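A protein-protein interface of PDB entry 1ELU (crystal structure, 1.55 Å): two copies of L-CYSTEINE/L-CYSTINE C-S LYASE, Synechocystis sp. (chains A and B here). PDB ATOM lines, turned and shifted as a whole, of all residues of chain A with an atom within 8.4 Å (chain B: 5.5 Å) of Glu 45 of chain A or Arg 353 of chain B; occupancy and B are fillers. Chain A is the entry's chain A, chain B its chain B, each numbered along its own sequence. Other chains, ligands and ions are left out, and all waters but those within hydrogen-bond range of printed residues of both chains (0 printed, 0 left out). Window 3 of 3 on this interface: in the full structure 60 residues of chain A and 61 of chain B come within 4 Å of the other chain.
No position is printed for both chains.
Of the 10 pairs that touch across the chains among the printed residues, none has its exchanged pair printed and touching as well.
Tyr 355 of chain B touches Asn 46 of chain A.
Gly 47 of chain A touches Lys 17 of chain B (O to CE, 3.7 Å).
Gly 47 of chain A touches Tyr 19 of chain B.
Pro 48 of chain A touches Tyr 19 of chain B (CD to OH, 3.5 Å).
OE2 of Glu 350 of chain B touches CB of Ser 50 of chain A (3.5 Å).
Ser 50 of chain A touches Tyr 355 of chain B (CB to CD2, 3.4 Å).
Of the 14 printed residues of chain A, 7 touch a printed residue of chain B.
Hydrophobic or aromatic side chains of chain A that line the printed part of chain B: Pro 48 and Ala 52.
Hydrophobic or aromatic side chains of chain B within 4 Å of the printed part of chain A: Tyr 19 and Tyr 355.
NZ of Lys 17 of chain B is in hydrogen-bond range of O of Glu 45 of chain A, 3.3 Å away.
OE1 of Glu 45 of chain A lies within salt-bridge range of NH2 of Arg 353 of chain B, 3.4 Å away.
N of Ala 52 of chain A lies within hydrogen-bond range of OE1 of Glu 350 of chain B.
O of Gln 44 of chain A sits at hydrogen-bond distance from NZ of Lys 17 of chain B (2.8 Å).
The side-chain amide oxygen of Asn 46 of chain A lies close to the side-chain carboxylate of Glu 45 of chain A.
O of Tyr 42 of chain A sits at hydrogen-bond distance from ND2 of Asn 46 of chain A.
The backbone NH (N) of Thr 18 of chain B is in hydrogen-bond range of the backbone carbonyl oxygen (O) of Arg 353 of chain B.
The side-chain hydroxyl (OG) of Ser 50 of chain A sits at hydrogen-bond distance from the backbone carbonyl oxygen (O) of Asn 46 of chain A (2.7 Å).
The backbone carbonyl oxygen of Thr 18 of chain B lies within hydrogen-bond range of the backbone NH of Tyr 355 of chain B, 2.9 Å away.
The side-chain hydroxyl (OG) of Ser 50 of chain A is in hydrogen-bond range of the backbone NH (N) of Ala 53 of chain A (2.9 Å).
Of the printed residues of chain B, Gly 47 of chain A touches Lys 17 (3.7 Å) and Tyr 19 (3.4 Å).
Of the printed residues of chain B, Ala 52 of chain A touches Glu 350 (2.9 Å).
Of the printed residues of chain A, Tyr 355 of chain B touches Asn 46 (3.6 Å) and Ser 50 (3.4 Å).
Of the printed residues of chain B, Asn 46 of chain A touches Tyr 355 (3.6 Å).
Gly 41 of chain A touches none of the printed residues of chain B.
Met 39 of chain A touches none of the printed residues of chain B.
The nearest printed residue of chain B that does not touch Asn 46 of chain A is Lys 17 of chain B (4.7 Å).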
ATOM      1  N   ALA A  38       5.080  31.306   4.108  1.00  0.00           N
ATOM      2  CA  ALA A  38       4.259  30.333   4.830  1.00  0.00           C
ATOM      3  C   ALA A  38       3.009  29.963   4.061  1.00  0.00           C
ATOM      4  O   ALA A  38       2.549  28.825   4.143  1.00  0.00           O
ATOM      5  CB  ALA A  38       3.872  30.861   6.213  1.00  0.00           C
ATOM      6  N   MET A  39       2.452  30.916   3.323  1.00  0.00           N
ATOM      7  CA  MET A  39       1.259  30.652   2.515  1.00  0.00           C
ATOM      8  C   MET A  39       1.567  29.713   1.335  1.00  0.00           C
ATOM      9  O   MET A  39       0.763  28.818   1.038  1.00  0.00           O
ATOM     10  CB  MET A  39       0.650  31.958   1.996  1.00  0.00           C
ATOM     11  CG  MET A  39      -0.622  32.373   2.723  1.00  0.00           C
ATOM     12  SD  MET A  39      -1.968  31.146   2.747  1.00  0.00           S
ATOM     13  CE  MET A  39      -2.483  31.109   1.085  1.00  0.00           C
ATOM     14  N   TYR A  40       2.713  29.881   0.672  1.00  0.00           N
ATOM     15  CA  TYR A  40       3.029  28.946  -0.420  1.00  0.00           C
ATOM     16  C   TYR A  40       3.127  27.566   0.198  1.00  0.00           C
ATOM     17  O   TYR A  40       2.635  26.592  -0.350  1.00  0.00           O
ATOM     18  CB  TYR A  40       4.360  29.287  -1.085  1.00  0.00           C
ATOM     19  CG  TYR A  40       4.251  30.387  -2.098  1.00  0.00           C
ATOM     20  CD1 TYR A  40       4.832  31.629  -1.877  1.00  0.00           C
ATOM     21  CD2 TYR A  40       3.547  30.189  -3.304  1.00  0.00           C
ATOM     22  CE1 TYR A  40       4.728  32.655  -2.826  1.00  0.00           C
ATOM     23  CE2 TYR A  40       3.435  31.186  -4.227  1.00  0.00           C
ATOM     24  CZ  TYR A  40       4.021  32.414  -3.997  1.00  0.00           C
ATOM     25  OH  TYR A  40       3.930  33.439  -4.903  1.00  0.00           O
ATOM     26  N   GLY A  41       3.738  27.503   1.374  1.00  0.00           N
ATOM     27  CA  GLY A  41       3.881  26.229   2.055  1.00  0.00           C
ATOM     28  C   GLY A  41       2.544  25.598   2.395  1.00  0.00           C
ATOM     29  O   GLY A  41       2.356  24.383   2.219  1.00  0.00           O
ATOM     30  N   TYR A  42       1.611  26.408   2.899  1.00  0.00           N
ATOM     31  CA  TYR A  42       0.298  25.902   3.243  1.00  0.00           C
ATOM     32  C   TYR A  42      -0.349  25.330   1.986  1.00  0.00           C
ATOM     33  O   TYR A  42      -0.912  24.241   2.011  1.00  0.00           O
ATOM     34  CB  TYR A  42      -0.600  27.009   3.809  1.00  0.00           C
ATOM     35  CG  TYR A  42      -1.938  26.466   4.254  1.00  0.00           C
ATOM     36  CD1 TYR A  42      -2.930  26.140   3.323  1.00  0.00           C
ATOM     37  CD2 TYR A  42      -2.196  26.234   5.606  1.00  0.00           C
ATOM     38  CE1 TYR A  42      -4.140  25.594   3.724  1.00  0.00           C
ATOM     39  CE2 TYR A  42      -3.402  25.693   6.021  1.00  0.00           C
ATOM     40  CZ  TYR A  42      -4.369  25.374   5.074  1.00  0.00           C
ATOM     41  OH  TYR A  42      -5.565  24.827   5.473  1.00  0.00           O
ATOM     42  N   LEU A  43      -0.269  26.065   0.881  1.00  0.00           N
ATOM     43  CA  LEU A  43      -0.857  25.596  -0.372  1.00  0.00           C
ATOM     44  C   LEU A  43      -0.208  24.298  -0.867  1.00  0.00           C
ATOM     45  O   LEU A  43      -0.900  23.398  -1.339  1.00  0.00           O
ATOM     46  CB  LEU A  43      -0.761  26.682  -1.464  1.00  0.00           C
ATOM     47  CG  LEU A  43      -1.654  27.917  -1.321  1.00  0.00           C
ATOM     48  CD1 LEU A  43      -1.381  28.896  -2.487  1.00  0.00           C
ATOM     49  CD2 LEU A  43      -3.115  27.489  -1.348  1.00  0.00           C
ATOM     50  N   GLN A  44       1.108  24.191  -0.762  1.00  0.00           N
ATOM     51  CA  GLN A  44       1.765  22.978  -1.231  1.00  0.00           C
ATOM     52  C   GLN A  44       1.356  21.806  -0.362  1.00  0.00           C
ATOM     53  O   GLN A  44       1.094  20.711  -0.853  1.00  0.00           O
ATOM     54  CB  GLN A  44       3.293  23.127  -1.206  1.00  0.00           C
ATOM     55  CG  GLN A  44       4.056  21.799  -1.423  1.00  0.00           C
ATOM     56  CD  GLN A  44       5.576  21.972  -1.520  1.00  0.00           C
ATOM     57  OE1 GLN A  44       6.106  22.457  -2.532  1.00  0.00           O
ATOM     58  NE2 GLN A  44       6.285  21.564  -0.467  1.00  0.00           N
ATOM     59  N   GLU A  45       1.267  22.046   0.939  1.00  0.00           N
ATOM     60  CA  GLU A  45       0.935  20.983   1.866  1.00  0.00           C
ATOM     61  C   GLU A  45      -0.503  20.488   1.796  1.00  0.00           C
ATOM     62  O   GLU A  45      -0.764  19.290   1.850  1.00  0.00           O
ATOM     63  CB  GLU A  45       1.238  21.456   3.299  1.00  0.00           C
ATOM     64  CG  GLU A  45       1.445  20.325   4.319  1.00  0.00           C
ATOM     65  CD  GLU A  45       0.206  19.465   4.554  1.00  0.00           C
ATOM     66  OE1 GLU A  45       0.371  18.270   4.908  1.00  0.00           O
ATOM     67  OE2 GLU A  45      -0.927  19.979   4.406  1.00  0.00           O
ATOM     68  N   ASN A  46      -1.438  21.421   1.668  1.00  0.00           N
ATOM     69  CA  ASN A  46      -2.847  21.115   1.704  1.00  0.00           C
ATOM     70  C   ASN A  46      -3.650  21.200   0.428  1.00  0.00           C
ATOM     71  O   ASN A  46      -4.847  20.923   0.450  1.00  0.00           O
ATOM     72  CB  ASN A  46      -3.513  22.050   2.733  1.00  0.00           C
ATOM     73  CG  ASN A  46      -2.941  21.868   4.129  1.00  0.00           C
ATOM     74  OD1 ASN A  46      -3.240  20.882   4.806  1.00  0.00           O
ATOM     75  ND2 ASN A  46      -2.094  22.806   4.557  1.00  0.00           N
ATOM     76  N   GLY A  47      -3.000  21.576  -0.671  1.00  0.00           N
ATOM     77  CA  GLY A  47      -3.723  21.717  -1.926  1.00  0.00           C
ATOM     78  C   GLY A  47      -2.790  21.546  -3.111  1.00  0.00           C
ATOM     79  O   GLY A  47      -2.134  20.518  -3.215  1.00  0.00           O
ATOM     80  N   PRO A  48      -2.552  22.600  -3.902  1.00  0.00           N
ATOM     81  CA  PRO A  48      -3.063  23.967  -3.777  1.00  0.00           C
ATOM     82  C   PRO A  48      -4.533  24.245  -3.982  1.00  0.00           C
ATOM     83  O   PRO A  48      -5.032  25.302  -3.551  1.00  0.00           O
ATOM     84  CB  PRO A  48      -2.152  24.763  -4.724  1.00  0.00           C
ATOM     85  CG  PRO A  48      -1.842  23.759  -5.819  1.00  0.00           C
ATOM     86  CD  PRO A  48      -1.642  22.465  -5.051  1.00  0.00           C
ATOM     87  N   SER A  50      -8.143  22.637  -3.188  1.00  0.00           N
ATOM     88  CA  SER A  50      -8.822  21.636  -2.377  1.00  0.00           C
ATOM     89  C   SER A  50      -9.820  22.367  -1.485  1.00  0.00           C
ATOM     90  O   SER A  50      -9.835  23.590  -1.441  1.00  0.00           O
ATOM     91  CB  SER A  50      -7.805  20.935  -1.481  1.00  0.00           C
ATOM     92  OG  SER A  50      -7.162  21.854  -0.585  1.00  0.00           O
ATOM     93  N   ALA A  52      -9.796  22.340   1.778  1.00  0.00           N
ATOM     94  CA  ALA A  52      -9.007  22.975   2.842  1.00  0.00           C
ATOM     95  C   ALA A  52      -8.302  24.228   2.359  1.00  0.00           C
ATOM     96  O   ALA A  52      -8.363  25.282   3.000  1.00  0.00           O
ATOM     97  CB  ALA A  52      -7.978  21.992   3.412  1.00  0.00           C
ATOM     98  N   ALA A  53      -7.629  24.128   1.220  1.00  0.00           N
ATOM     99  CA  ALA A  53      -6.887  25.287   0.720  1.00  0.00           C
ATOM    100  C   ALA A  53      -7.806  26.439   0.320  1.00  0.00           C
ATOM    101  O   ALA A  53      -7.507  27.603   0.621  1.00  0.00           O
ATOM    102  CB  ALA A  53      -5.999  24.885  -0.460  1.00  0.00           C
ATOM    103  N   ALA B  15       4.093  14.366  -3.222  1.00  0.00           N
ATOM    104  CA  ALA B  15       4.330  13.364  -2.190  1.00  0.00           C
ATOM    105  C   ALA B  15       3.330  13.441  -1.038  1.00  0.00           C
ATOM    106  O   ALA B  15       2.925  14.523  -0.605  1.00  0.00           O
ATOM    107  CB  ALA B  15       5.752  13.501  -1.672  1.00  0.00           C
ATOM    108  N   ASN B  16       2.912  12.276  -0.559  1.00  0.00           N
ATOM    109  CA  ASN B  16       1.982  12.201   0.560  1.00  0.00           C
ATOM    110  C   ASN B  16       0.557  12.708   0.317  1.00  0.00           C
ATOM    111  O   ASN B  16      -0.195  12.993   1.255  1.00  0.00           O
ATOM    112  CB  ASN B  16       2.609  12.856   1.796  1.00  0.00           C
ATOM    113  CG  ASN B  16       3.842  12.092   2.291  1.00  0.00           C
ATOM    114  OD1 ASN B  16       4.982  12.538   2.110  1.00  0.00           O
ATOM    115  ND2 ASN B  16       3.615  10.926   2.902  1.00  0.00           N
ATOM    116  N   LYS B  17       0.197  12.821  -0.956  1.00  0.00           N
ATOM    117  CA  LYS B  17      -1.162  13.150  -1.344  1.00  0.00           C
ATOM    118  C   LYS B  17      -1.393  12.475  -2.695  1.00  0.00           C
ATOM    119  O   LYS B  17      -0.445  11.967  -3.309  1.00  0.00           O
ATOM    120  CB  LYS B  17      -1.405  14.677  -1.382  1.00  0.00           C
ATOM    121  CG  LYS B  17      -0.628  15.475  -2.393  1.00  0.00           C
ATOM    122  CD  LYS B  17      -1.142  16.940  -2.441  1.00  0.00           C
ATOM    123  CE  LYS B  17      -0.913  17.697  -1.129  1.00  0.00           C
ATOM    124  NZ  LYS B  17       0.505  18.016  -0.885  1.00  0.00           N
ATOM    125  N   THR B  18      -2.649  12.391  -3.110  1.00  0.00           N
ATOM    126  CA  THR B  18      -3.010  11.781  -4.391  1.00  0.00           C
ATOM    127  C   THR B  18      -3.818  12.883  -5.067  1.00  0.00           C
ATOM    128  O   THR B  18      -5.038  12.981  -4.901  1.00  0.00           O
ATOM    129  CB  THR B  18      -3.828  10.516  -4.173  1.00  0.00           C
ATOM    130  OG1 THR B  18      -3.065   9.611  -3.349  1.00  0.00           O
ATOM    131  CG2 THR B  18      -4.128   9.838  -5.535  1.00  0.00           C
ATOM    132  N   TYR B  19      -3.105  13.676  -5.869  1.00  0.00           N
ATOM    133  CA  TYR B  19      -3.641  14.885  -6.495  1.00  0.00           C
ATOM    134  C   TYR B  19      -4.201  14.791  -7.890  1.00  0.00           C
ATOM    135  O   TYR B  19      -3.470  14.427  -8.814  1.00  0.00           O
ATOM    136  CB  TYR B  19      -2.542  15.955  -6.480  1.00  0.00           C
ATOM    137  CG  TYR B  19      -3.048  17.390  -6.599  1.00  0.00           C
ATOM    138  CD1 TYR B  19      -2.867  18.132  -7.772  1.00  0.00           C
ATOM    139  CD2 TYR B  19      -3.706  18.009  -5.536  1.00  0.00           C
ATOM    140  CE1 TYR B  19      -3.340  19.462  -7.881  1.00  0.00           C
ATOM    141  CE2 TYR B  19      -4.158  19.304  -5.622  1.00  0.00           C
ATOM    142  CZ  TYR B  19      -3.981  20.035  -6.783  1.00  0.00           C
ATOM    143  OH  TYR B  19      -4.370  21.338  -6.869  1.00  0.00           O
ATOM    144  N   LEU B 349     -13.064  11.831   0.100  1.00  0.00           N
ATOM    145  CA  LEU B 349     -11.824  11.553  -0.591  1.00  0.00           C
ATOM    146  C   LEU B 349     -10.703  12.482  -0.090  1.00  0.00           C
ATOM    147  O   LEU B 349      -9.584  12.049   0.079  1.00  0.00           O
ATOM    148  CB  LEU B 349     -12.004  11.699  -2.107  1.00  0.00           C
ATOM    149  CG  LEU B 349     -12.819  10.605  -2.787  1.00  0.00           C
ATOM    150  CD1 LEU B 349     -13.064  11.023  -4.271  1.00  0.00           C
ATOM    151  CD2 LEU B 349     -12.065   9.263  -2.698  1.00  0.00           C
ATOM    152  N   GLU B 350     -11.012  13.756   0.150  1.00  0.00           N
ATOM    153  CA  GLU B 350     -10.018  14.694   0.634  1.00  0.00           C
ATOM    154  C   GLU B 350      -9.583  14.325   2.064  1.00  0.00           C
ATOM    155  O   GLU B 350      -8.431  14.539   2.451  1.00  0.00           O
ATOM    156  CB  GLU B 350     -10.568  16.132   0.572  1.00  0.00           C
ATOM    157  CG  GLU B 350      -9.593  17.118   1.157  1.00  0.00           C
ATOM    158  CD  GLU B 350      -9.801  18.581   0.755  1.00  0.00           C
ATOM    159  OE1 GLU B 350      -9.372  19.445   1.544  1.00  0.00           O
ATOM    160  OE2 GLU B 350     -10.346  18.879  -0.322  1.00  0.00           O
ATOM    161  N   GLU B 351     -10.496  13.730   2.827  1.00  0.00           N
ATOM    162  CA  GLU B 351     -10.197  13.278   4.180  1.00  0.00           C
ATOM    163  C   GLU B 351      -9.084  12.202   4.071  1.00  0.00           C
ATOM    164  O   GLU B 351      -8.280  12.008   4.986  1.00  0.00           O
ATOM    165  CB  GLU B 351     -11.493  12.716   4.801  1.00  0.00           C
ATOM    166  CG  GLU B 351     -11.619  12.796   6.322  1.00  0.00           C
ATOM    167  CD  GLU B 351     -11.682  14.227   6.841  1.00  0.00           C
ATOM    168  OE1 GLU B 351     -10.608  14.849   7.003  1.00  0.00           O
ATOM    169  OE2 GLU B 351     -12.803  14.740   7.085  1.00  0.00           O
ATOM    170  N   GLN B 352      -8.996  11.543   2.912  1.00  0.00           N
ATOM    171  CA  GLN B 352      -7.962  10.513   2.690  1.00  0.00           C
ATOM    172  C   GLN B 352      -6.800  11.061   1.847  1.00  0.00           C
ATOM    173  O   GLN B 352      -5.961  10.298   1.329  1.00  0.00           O
ATOM    174  CB  GLN B 352      -8.595   9.306   1.977  1.00  0.00           C
ATOM    175  CG  GLN B 352      -9.736   8.682   2.776  1.00  0.00           C
ATOM    176  CD  GLN B 352     -10.551   7.713   1.964  1.00  0.00           C
ATOM    177  OE1 GLN B 352     -10.133   6.580   1.716  1.00  0.00           O
ATOM    178  NE2 GLN B 352     -11.715   8.157   1.523  1.00  0.00           N
ATOM    179  N   ARG B 353      -6.752  12.379   1.730  1.00  0.00           N
ATOM    180  CA  ARG B 353      -5.744  13.089   0.959  1.00  0.00           C
ATOM    181  C   ARG B 353      -5.722  12.725  -0.523  1.00  0.00           C
ATOM    182  O   ARG B 353      -4.661  12.635  -1.137  1.00  0.00           O
ATOM    183  CB  ARG B 353      -4.356  12.948   1.609  1.00  0.00           C
ATOM    184  CG  ARG B 353      -4.295  13.588   3.016  1.00  0.00           C
ATOM    185  CD  ARG B 353      -2.879  13.506   3.623  1.00  0.00           C
ATOM    186  NE  ARG B 353      -1.926  14.369   2.929  1.00  0.00           N
ATOM    187  CZ  ARG B 353      -1.864  15.690   3.071  1.00  0.00           C
ATOM    188  NH1 ARG B 353      -2.697  16.311   3.896  1.00  0.00           N
ATOM    189  NH2 ARG B 353      -0.976  16.391   2.373  1.00  0.00           N
ATOM    190  N   ILE B 354      -6.921  12.543  -1.063  1.00  0.00           N
ATOM    191  CA  ILE B 354      -7.173  12.270  -2.486  1.00  0.00           C
ATOM    192  C   ILE B 354      -7.983  13.503  -2.924  1.00  0.00           C
ATOM    193  O   ILE B 354      -9.091  13.790  -2.398  1.00  0.00           O
ATOM    194  CB  ILE B 354      -7.943  10.963  -2.683  1.00  0.00           C
ATOM    195  CG1 ILE B 354      -7.117   9.799  -2.132  1.00  0.00           C
ATOM    196  CG2 ILE B 354      -8.175  10.741  -4.153  1.00  0.00           C
ATOM    197  CD1 ILE B 354      -7.860   8.469  -2.043  1.00  0.00           C
ATOM    198  N   TYR B 355      -7.423  14.247  -3.884  1.00  0.00           N
ATOM    199  CA  TYR B 355      -7.988  15.524  -4.285  1.00  0.00           C
ATOM    200  C   TYR B 355      -8.608  15.631  -5.667  1.00  0.00           C
ATOM    201  O   TYR B 355      -7.894  15.694  -6.649  1.00  0.00           O
ATOM    202  CB  TYR B 355      -6.900  16.593  -4.169  1.00  0.00           C
ATOM    203  CG  TYR B 355      -6.323  16.732  -2.772  1.00  0.00           C
ATOM    204  CD1 TYR B 355      -5.294  15.908  -2.317  1.00  0.00           C
ATOM    205  CD2 TYR B 355      -6.841  17.673  -1.896  1.00  0.00           C
ATOM    206  CE1 TYR B 355      -4.790  16.029  -1.000  1.00  0.00           C
ATOM    207  CE2 TYR B 355      -6.348  17.793  -0.590  1.00  0.00           C
ATOM    208  CZ  TYR B 355      -5.333  16.974  -0.159  1.00  0.00           C
ATOM    209  OH  TYR B 355      -4.857  17.097   1.125  1.00  0.00           O
